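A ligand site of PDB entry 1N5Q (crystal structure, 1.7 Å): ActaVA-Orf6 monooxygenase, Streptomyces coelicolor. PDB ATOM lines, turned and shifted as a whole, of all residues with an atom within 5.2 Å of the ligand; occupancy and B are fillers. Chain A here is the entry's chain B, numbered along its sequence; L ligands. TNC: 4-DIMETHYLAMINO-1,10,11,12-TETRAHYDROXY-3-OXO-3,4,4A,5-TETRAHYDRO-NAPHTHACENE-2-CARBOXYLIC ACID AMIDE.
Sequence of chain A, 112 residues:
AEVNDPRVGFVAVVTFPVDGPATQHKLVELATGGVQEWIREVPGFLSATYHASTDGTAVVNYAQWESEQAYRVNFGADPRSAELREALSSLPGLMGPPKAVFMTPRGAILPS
An oxygen (O1) of the ligand sits at hydrogen-bond distance from the indole nitrogen of Trp 65 (3.1 Å).
OH of Tyr 71 lies within hydrogen-bond range of O3 of the ligand (3.0 Å).
The backbone carbonyl oxygen (O) of Val 14 lies within hydrogen-bond range of the backbone NH (N) of Asn 61 (2.9 Å).
The side-chain hydroxyl (OG) of Ser 89 lies within hydrogen-bond range of the backbone carbonyl oxygen (O) of Arg 85 (2.7 Å).
N of Ala 63 is in hydrogen-bond range of O of Ala 12.
Ala 12 touches the ligand (CB to O2, 3.8 Å).
CG2 of Val 14 touches O3 of the ligand, at 3.3 Å.
CE2 of Phe 16 touches C21 of the ligand, 3.4 Å away.
Ala 48 touches the ligand.
OH of Tyr 50 touches C1 of the ligand, 3.7 Å away.
Asn 61 touches the ligand.
Ala 63 touches the ligand (CB to O1, 3.3 Å).
Phe 75 touches the ligand (CZ to C2, 3.8 Å).
Arg 85 touches the ligand (CG to N1, 3.0 Å).
Leu 88 touches the ligand.
CB of Ser 89 touches C20 of the ligand (3.3 Å).
Pro 98 touches the ligand.
CB of Ala 100 touches O4 of the ligand (3.5 Å).
Hydrophobic or aromatic side chains that line the ligand: Ala 12, Val 14, Phe 16, Ala 48, Ala 63, Trp 65, Tyr 71, Phe 75, Leu 88, Pro 98 and Ala 100.
15 residues have an atom within 4 Å of the ligand: Ala 12, Val 14, Phe 16, Ala 48, Tyr 50, Asn 61, Ala 63, Trp 65, Tyr 71, Phe 75, Arg 85, Leu 88, Ser 89, Pro 98 and Ala 100.
Along chain A the residues within 4 Å of the ligand span positions 12 to 100.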
ATOM      1  N   ALA A  12      14.068   0.660 -17.404  1.00  0.00           N
ATOM      2  CA  ALA A  12      15.461   0.542 -18.001  1.00  0.00           C
ATOM      3  C   ALA A  12      16.281  -0.094 -16.903  1.00  0.00           C
ATOM      4  O   ALA A  12      16.150   0.246 -15.691  1.00  0.00           O
ATOM      5  CB  ALA A  12      16.015   1.877 -18.349  1.00  0.00           C
ATOM      6  N   VAL A  14      20.209  -0.598 -16.066  1.00  0.00           N
ATOM      7  CA  VAL A  14      21.510  -0.122 -16.564  1.00  0.00           C
ATOM      8  C   VAL A  14      22.578  -0.684 -15.639  1.00  0.00           C
ATOM      9  O   VAL A  14      22.530  -0.465 -14.435  1.00  0.00           O
ATOM     10  CB  VAL A  14      21.541   1.414 -16.531  1.00  0.00           C
ATOM     11  CG1 VAL A  14      22.878   1.878 -17.152  1.00  0.00           C
ATOM     12  CG2 VAL A  14      20.369   2.043 -17.291  1.00  0.00           C
ATOM     13  N   PHE A  16      26.591  -0.971 -14.622  1.00  0.00           N
ATOM     14  CA  PHE A  16      27.915  -0.297 -14.702  1.00  0.00           C
ATOM     15  C   PHE A  16      28.961  -1.220 -14.125  1.00  0.00           C
ATOM     16  O   PHE A  16      28.943  -1.481 -12.912  1.00  0.00           O
ATOM     17  CB  PHE A  16      27.876   0.938 -13.774  1.00  0.00           C
ATOM     18  CG  PHE A  16      26.838   1.972 -14.147  1.00  0.00           C
ATOM     19  CD1 PHE A  16      25.557   1.904 -13.680  1.00  0.00           C
ATOM     20  CD2 PHE A  16      27.180   2.988 -15.042  1.00  0.00           C
ATOM     21  CE1 PHE A  16      24.589   2.840 -14.002  1.00  0.00           C
ATOM     22  CE2 PHE A  16      26.204   3.918 -15.409  1.00  0.00           C
ATOM     23  CZ  PHE A  16      24.948   3.852 -14.864  1.00  0.00           C
ATOM     24  N   ILE A  39      15.906  15.006 -12.011  1.00  0.00           N
ATOM     25  CA  ILE A  39      15.299  13.803 -12.571  1.00  0.00           C
ATOM     26  C   ILE A  39      13.932  13.571 -11.927  1.00  0.00           C
ATOM     27  O   ILE A  39      12.978  13.065 -12.522  1.00  0.00           O
ATOM     28  CB  ILE A  39      16.255  12.616 -12.329  1.00  0.00           C
ATOM     29  CG1 ILE A  39      17.600  12.874 -13.003  1.00  0.00           C
ATOM     30  CG2 ILE A  39      15.593  11.337 -12.859  1.00  0.00           C
ATOM     31  CD1 ILE A  39      18.627  11.745 -12.843  1.00  0.00           C
ATOM     32  N   PHE A  45       8.709  10.347 -15.100  1.00  0.00           N
ATOM     33  CA  PHE A  45       9.665   9.594 -14.248  1.00  0.00           C
ATOM     34  C   PHE A  45       8.936   9.032 -13.036  1.00  0.00           C
ATOM     35  O   PHE A  45       8.192   9.758 -12.337  1.00  0.00           O
ATOM     36  CB  PHE A  45      10.817  10.506 -13.751  1.00  0.00           C
ATOM     37  CG  PHE A  45      11.733   9.888 -12.723  1.00  0.00           C
ATOM     38  CD1 PHE A  45      12.657   8.923 -13.084  1.00  0.00           C
ATOM     39  CD2 PHE A  45      11.672  10.297 -11.384  1.00  0.00           C
ATOM     40  CE1 PHE A  45      13.513   8.334 -12.161  1.00  0.00           C
ATOM     41  CE2 PHE A  45      12.522   9.729 -10.458  1.00  0.00           C
ATOM     42  CZ  PHE A  45      13.449   8.761 -10.832  1.00  0.00           C
ATOM     43  N   SER A  47      10.798   6.237 -10.844  1.00  0.00           N
ATOM     44  CA  SER A  47      11.767   5.860  -9.822  1.00  0.00           C
ATOM     45  C   SER A  47      13.072   5.369 -10.452  1.00  0.00           C
ATOM     46  O   SER A  47      13.107   5.031 -11.661  1.00  0.00           O
ATOM     47  CB  SER A  47      11.278   4.683  -8.946  1.00  0.00           C
ATOM     48  OG  SER A  47      11.361   3.470  -9.767  1.00  0.00           O
ATOM     49  N   ALA A  48      14.153   5.546  -9.670  1.00  0.00           N
ATOM     50  CA  ALA A  48      15.453   4.998 -10.109  1.00  0.00           C
ATOM     51  C   ALA A  48      16.076   4.403  -8.852  1.00  0.00           C
ATOM     52  O   ALA A  48      16.217   5.158  -7.870  1.00  0.00           O
ATOM     53  CB  ALA A  48      16.360   6.005 -10.771  1.00  0.00           C
ATOM     54  N   TYR A  50      19.370   2.443  -7.226  1.00  0.00           N
ATOM     55  CA  TYR A  50      20.698   1.925  -7.540  1.00  0.00           C
ATOM     56  C   TYR A  50      21.070   0.816  -6.567  1.00  0.00           C
ATOM     57  O   TYR A  50      20.815   0.932  -5.344  1.00  0.00           O
ATOM     58  CB  TYR A  50      21.748   3.079  -7.416  1.00  0.00           C
ATOM     59  CG  TYR A  50      21.683   4.016  -8.607  1.00  0.00           C
ATOM     60  CD1 TYR A  50      20.726   5.021  -8.711  1.00  0.00           C
ATOM     61  CD2 TYR A  50      22.597   3.858  -9.631  1.00  0.00           C
ATOM     62  CE1 TYR A  50      20.710   5.838  -9.836  1.00  0.00           C
ATOM     63  CE2 TYR A  50      22.592   4.671 -10.746  1.00  0.00           C
ATOM     64  CZ  TYR A  50      21.638   5.657 -10.840  1.00  0.00           C
ATOM     65  OH  TYR A  50      21.613   6.440 -11.976  1.00  0.00           O
ATOM     66  N   ASN A  61      21.149   0.016 -11.972  1.00  0.00           N
ATOM     67  CA  ASN A  61      20.019   0.945 -11.786  1.00  0.00           C
ATOM     68  C   ASN A  61      18.764   0.307 -12.420  1.00  0.00           C
ATOM     69  O   ASN A  61      18.797  -0.017 -13.611  1.00  0.00           O
ATOM     70  CB  ASN A  61      20.350   2.266 -12.490  1.00  0.00           C
ATOM     71  CG  ASN A  61      19.172   3.251 -12.555  1.00  0.00           C
ATOM     72  OD1 ASN A  61      18.170   3.081 -11.877  1.00  0.00           O
ATOM     73  ND2 ASN A  61      19.263   4.264 -13.406  1.00  0.00           N
ATOM     74  N   ALA A  63      15.119   1.370 -13.267  1.00  0.00           N
ATOM     75  CA  ALA A  63      14.382   2.660 -13.306  1.00  0.00           C
ATOM     76  C   ALA A  63      12.992   2.446 -13.903  1.00  0.00           C
ATOM     77  O   ALA A  63      12.837   1.781 -14.925  1.00  0.00           O
ATOM     78  CB  ALA A  63      15.133   3.667 -14.211  1.00  0.00           C
ATOM     79  N   TRP A  65       9.539   4.121 -15.524  1.00  0.00           N
ATOM     80  CA  TRP A  65       9.036   5.234 -16.313  1.00  0.00           C
ATOM     81  C   TRP A  65       7.594   4.961 -16.663  1.00  0.00           C
ATOM     82  O   TRP A  65       7.209   3.801 -16.805  1.00  0.00           O
ATOM     83  CB  TRP A  65       9.855   5.384 -17.624  1.00  0.00           C
ATOM     84  CG  TRP A  65      11.237   5.899 -17.280  1.00  0.00           C
ATOM     85  CD1 TRP A  65      12.315   5.151 -16.936  1.00  0.00           C
ATOM     86  CD2 TRP A  65      11.599   7.277 -17.177  1.00  0.00           C
ATOM     87  NE1 TRP A  65      13.375   6.023 -16.626  1.00  0.00           N
ATOM     88  CE2 TRP A  65      12.933   7.298 -16.779  1.00  0.00           C
ATOM     89  CE3 TRP A  65      10.862   8.453 -17.395  1.00  0.00           C
ATOM     90  CZ2 TRP A  65      13.625   8.518 -16.606  1.00  0.00           C
ATOM     91  CZ3 TRP A  65      11.552   9.675 -17.208  1.00  0.00           C
ATOM     92  CH2 TRP A  65      12.896   9.642 -16.807  1.00  0.00           C
ATOM     93  N   TYR A  71      10.540   8.496 -21.402  1.00  0.00           N
ATOM     94  CA  TYR A  71      11.947   8.310 -21.205  1.00  0.00           C
ATOM     95  C   TYR A  71      12.727   8.905 -22.375  1.00  0.00           C
ATOM     96  O   TYR A  71      13.715   9.604 -22.162  1.00  0.00           O
ATOM     97  CB  TYR A  71      12.259   6.773 -21.161  1.00  0.00           C
ATOM     98  CG  TYR A  71      13.748   6.482 -21.172  1.00  0.00           C
ATOM     99  CD1 TYR A  71      14.425   6.573 -19.954  1.00  0.00           C
ATOM    100  CD2 TYR A  71      14.441   6.134 -22.313  1.00  0.00           C
ATOM    101  CE1 TYR A  71      15.765   6.282 -19.929  1.00  0.00           C
ATOM    102  CE2 TYR A  71      15.800   5.854 -22.293  1.00  0.00           C
ATOM    103  CZ  TYR A  71      16.450   5.962 -21.084  1.00  0.00           C
ATOM    104  OH  TYR A  71      17.791   5.704 -20.947  1.00  0.00           O
ATOM    105  N   PHE A  75      13.455  12.735 -20.834  1.00  0.00           N
ATOM    106  CA  PHE A  75      14.741  12.542 -20.223  1.00  0.00           C
ATOM    107  C   PHE A  75      15.830  12.540 -21.309  1.00  0.00           C
ATOM    108  O   PHE A  75      16.697  13.368 -21.272  1.00  0.00           O
ATOM    109  CB  PHE A  75      14.762  11.230 -19.427  1.00  0.00           C
ATOM    110  CG  PHE A  75      16.048  10.870 -18.715  1.00  0.00           C
ATOM    111  CD1 PHE A  75      16.481  11.543 -17.610  1.00  0.00           C
ATOM    112  CD2 PHE A  75      16.773   9.796 -19.180  1.00  0.00           C
ATOM    113  CE1 PHE A  75      17.659  11.152 -16.974  1.00  0.00           C
ATOM    114  CE2 PHE A  75      17.971   9.402 -18.554  1.00  0.00           C
ATOM    115  CZ  PHE A  75      18.411  10.074 -17.426  1.00  0.00           C
ATOM    116  N   LEU A  84      24.808  13.884 -17.437  1.00  0.00           N
ATOM    117  CA  LEU A  84      24.859  12.852 -16.416  1.00  0.00           C
ATOM    118  C   LEU A  84      25.549  11.599 -16.955  1.00  0.00           C
ATOM    119  O   LEU A  84      26.418  11.028 -16.294  1.00  0.00           O
ATOM    120  CB  LEU A  84      23.404  12.518 -16.015  1.00  0.00           C
ATOM    121  CG  LEU A  84      23.284  11.262 -15.132  1.00  0.00           C
ATOM    122  CD1 LEU A  84      23.965  11.469 -13.779  1.00  0.00           C
ATOM    123  CD2 LEU A  84      21.828  10.877 -14.993  1.00  0.00           C
ATOM    124  N   ARG A  85      25.214  11.243 -18.200  1.00  0.00           N
ATOM    125  CA  ARG A  85      25.880  10.121 -18.866  1.00  0.00           C
ATOM    126  C   ARG A  85      27.382  10.317 -18.958  1.00  0.00           C
ATOM    127  O   ARG A  85      28.122   9.369 -18.680  1.00  0.00           O
ATOM    128  CB  ARG A  85      25.257   9.866 -20.221  1.00  0.00           C
ATOM    129  CG  ARG A  85      24.213   8.781 -19.990  1.00  0.00           C
ATOM    130  CD  ARG A  85      23.045   9.335 -19.190  1.00  0.00           C
ATOM    131  NE  ARG A  85      21.786   9.140 -19.852  1.00  0.00           N
ATOM    132  CZ  ARG A  85      21.498   8.999 -21.136  1.00  0.00           C
ATOM    133  NH1 ARG A  85      22.349   8.986 -22.152  1.00  0.00           N
ATOM    134  NH2 ARG A  85      20.205   8.844 -21.453  1.00  0.00           N
ATOM    135  N   LEU A  88      28.799   9.953 -15.205  1.00  0.00           N
ATOM    136  CA  LEU A  88      28.848   8.606 -14.631  1.00  0.00           C
ATOM    137  C   LEU A  88      29.816   7.706 -15.374  1.00  0.00           C
ATOM    138  O   LEU A  88      30.648   7.020 -14.775  1.00  0.00           O
ATOM    139  CB  LEU A  88      27.478   7.913 -14.564  1.00  0.00           C
ATOM    140  CG  LEU A  88      26.381   8.572 -13.730  1.00  0.00           C
ATOM    141  CD1 LEU A  88      25.097   7.765 -13.570  1.00  0.00           C
ATOM    142  CD2 LEU A  88      26.891   8.834 -12.310  1.00  0.00           C
ATOM    143  N   SER A  89      29.735   7.748 -16.703  1.00  0.00           N
ATOM    144  CA  SER A  89      30.573   6.904 -17.554  1.00  0.00           C
ATOM    145  C   SER A  89      32.016   7.369 -17.686  1.00  0.00           C
ATOM    146  O   SER A  89      32.703   6.844 -18.581  1.00  0.00           O
ATOM    147  CB  SER A  89      29.926   6.776 -18.927  1.00  0.00           C
ATOM    148  OG  SER A  89      30.082   7.929 -19.735  1.00  0.00           O
ATOM    149  N   PRO A  98      28.659   1.560 -19.474  1.00  0.00           N
ATOM    150  CA  PRO A  98      27.397   1.068 -18.907  1.00  0.00           C
ATOM    151  C   PRO A  98      26.666   0.328 -20.003  1.00  0.00           C
ATOM    152  O   PRO A  98      26.877   0.593 -21.214  1.00  0.00           O
ATOM    153  CB  PRO A  98      26.631   2.324 -18.487  1.00  0.00           C
ATOM    154  CG  PRO A  98      27.625   3.419 -18.532  1.00  0.00           C
ATOM    155  CD  PRO A  98      28.675   3.045 -19.545  1.00  0.00           C
ATOM    156  N   ALA A 100      22.779  -0.915 -21.044  1.00  0.00           N
ATOM    157  CA  ALA A 100      21.384  -0.755 -20.636  1.00  0.00           C
ATOM    158  C   ALA A 100      20.555  -1.812 -21.337  1.00  0.00           C
ATOM    159  O   ALA A 100      20.795  -2.167 -22.510  1.00  0.00           O
ATOM    160  CB  ALA A 100      20.920   0.644 -21.076  1.00  0.00           C
ATOM    161  N   PHE A 102      16.439  -2.374 -22.095  1.00  0.00           N
ATOM    162  CA  PHE A 102      15.110  -1.701 -21.966  1.00  0.00           C
ATOM    163  C   PHE A 102      14.033  -2.796 -21.952  1.00  0.00           C
ATOM    164  O   PHE A 102      14.148  -3.719 -22.732  1.00  0.00           O
ATOM    165  CB  PHE A 102      14.902  -0.683 -23.111  1.00  0.00           C
ATOM    166  CG  PHE A 102      16.015   0.364 -22.993  1.00  0.00           C
ATOM    167  CD1 PHE A 102      15.946   1.271 -21.947  1.00  0.00           C
ATOM    168  CD2 PHE A 102      17.067   0.348 -23.873  1.00  0.00           C
ATOM    169  CE1 PHE A 102      17.009   2.177 -21.824  1.00  0.00           C
ATOM    170  CE2 PHE A 102      18.085   1.318 -23.726  1.00  0.00           C
ATOM    171  CZ  PHE A 102      18.051   2.215 -22.707  1.00  0.00           C
HETATM  172  C2  TNC L   1      19.466   7.099 -15.369  1.00  0.00           C
HETATM  173  C1  TNC L   1      18.947   7.723 -14.251  1.00  0.00           C
HETATM  174  C6  TNC L   1      17.602   7.619 -13.937  1.00  0.00           C
HETATM  175  C5  TNC L   1      16.732   6.873 -14.703  1.00  0.00           C
HETATM  176  C4  TNC L   1      17.257   6.227 -15.823  1.00  0.00           C
HETATM  177  C3  TNC L   1      18.602   6.331 -16.137  1.00  0.00           C
HETATM  178  O1  TNC L   1      16.428   5.463 -16.614  1.00  0.00           O
HETATM  179  C8  TNC L   1      21.310   6.551 -16.851  1.00  0.00           C
HETATM  180  C7  TNC L   1      20.839   7.040 -15.630  1.00  0.00           C
HETATM  181  C10 TNC L   1      19.132   5.690 -17.250  1.00  0.00           C
HETATM  182  C9  TNC L   1      20.446   5.800 -17.644  1.00  0.00           C
HETATM  183  O2  TNC L   1      18.237   4.951 -17.978  1.00  0.00           O
HETATM  184  C12 TNC L   1      23.115   6.008 -18.313  1.00  0.00           C
HETATM  185  C11 TNC L   1      22.670   6.256 -17.011  1.00  0.00           C
HETATM  186  C14 TNC L   1      20.945   5.141 -18.753  1.00  0.00           C
HETATM  187  C13 TNC L   1      22.282   5.243 -19.141  1.00  0.00           C
HETATM  188  O3  TNC L   1      20.093   4.385 -19.550  1.00  0.00           O
HETATM  189  C15 TNC L   1      24.456   6.016 -18.613  1.00  0.00           C
HETATM  190  C16 TNC L   1      24.953   5.591 -19.839  1.00  0.00           C
HETATM  191  C17 TNC L   1      24.119   4.876 -20.661  1.00  0.00           C
HETATM  192  C18 TNC L   1      22.794   4.711 -20.304  1.00  0.00           C
HETATM  193  O4  TNC L   1      22.055   3.969 -21.219  1.00  0.00           O
HETATM  194  C19 TNC L   1      24.675   4.327 -21.893  1.00  0.00           C
HETATM  195  O5  TNC L   1      26.285   5.801 -20.136  1.00  0.00           O
HETATM  196  N2  TNC L   1      25.793   4.929 -22.354  1.00  0.00           N
HETATM  197  O6  TNC L   1      24.224   3.402 -22.560  1.00  0.00           O
HETATM  198  N1  TNC L   1      25.343   6.915 -17.948  1.00  0.00           N
HETATM  199  C20 TNC L   1      26.704   6.473 -18.158  1.00  0.00           C
HETATM  200  C21 TNC L   1      25.008   6.859 -16.547  1.00  0.00           C
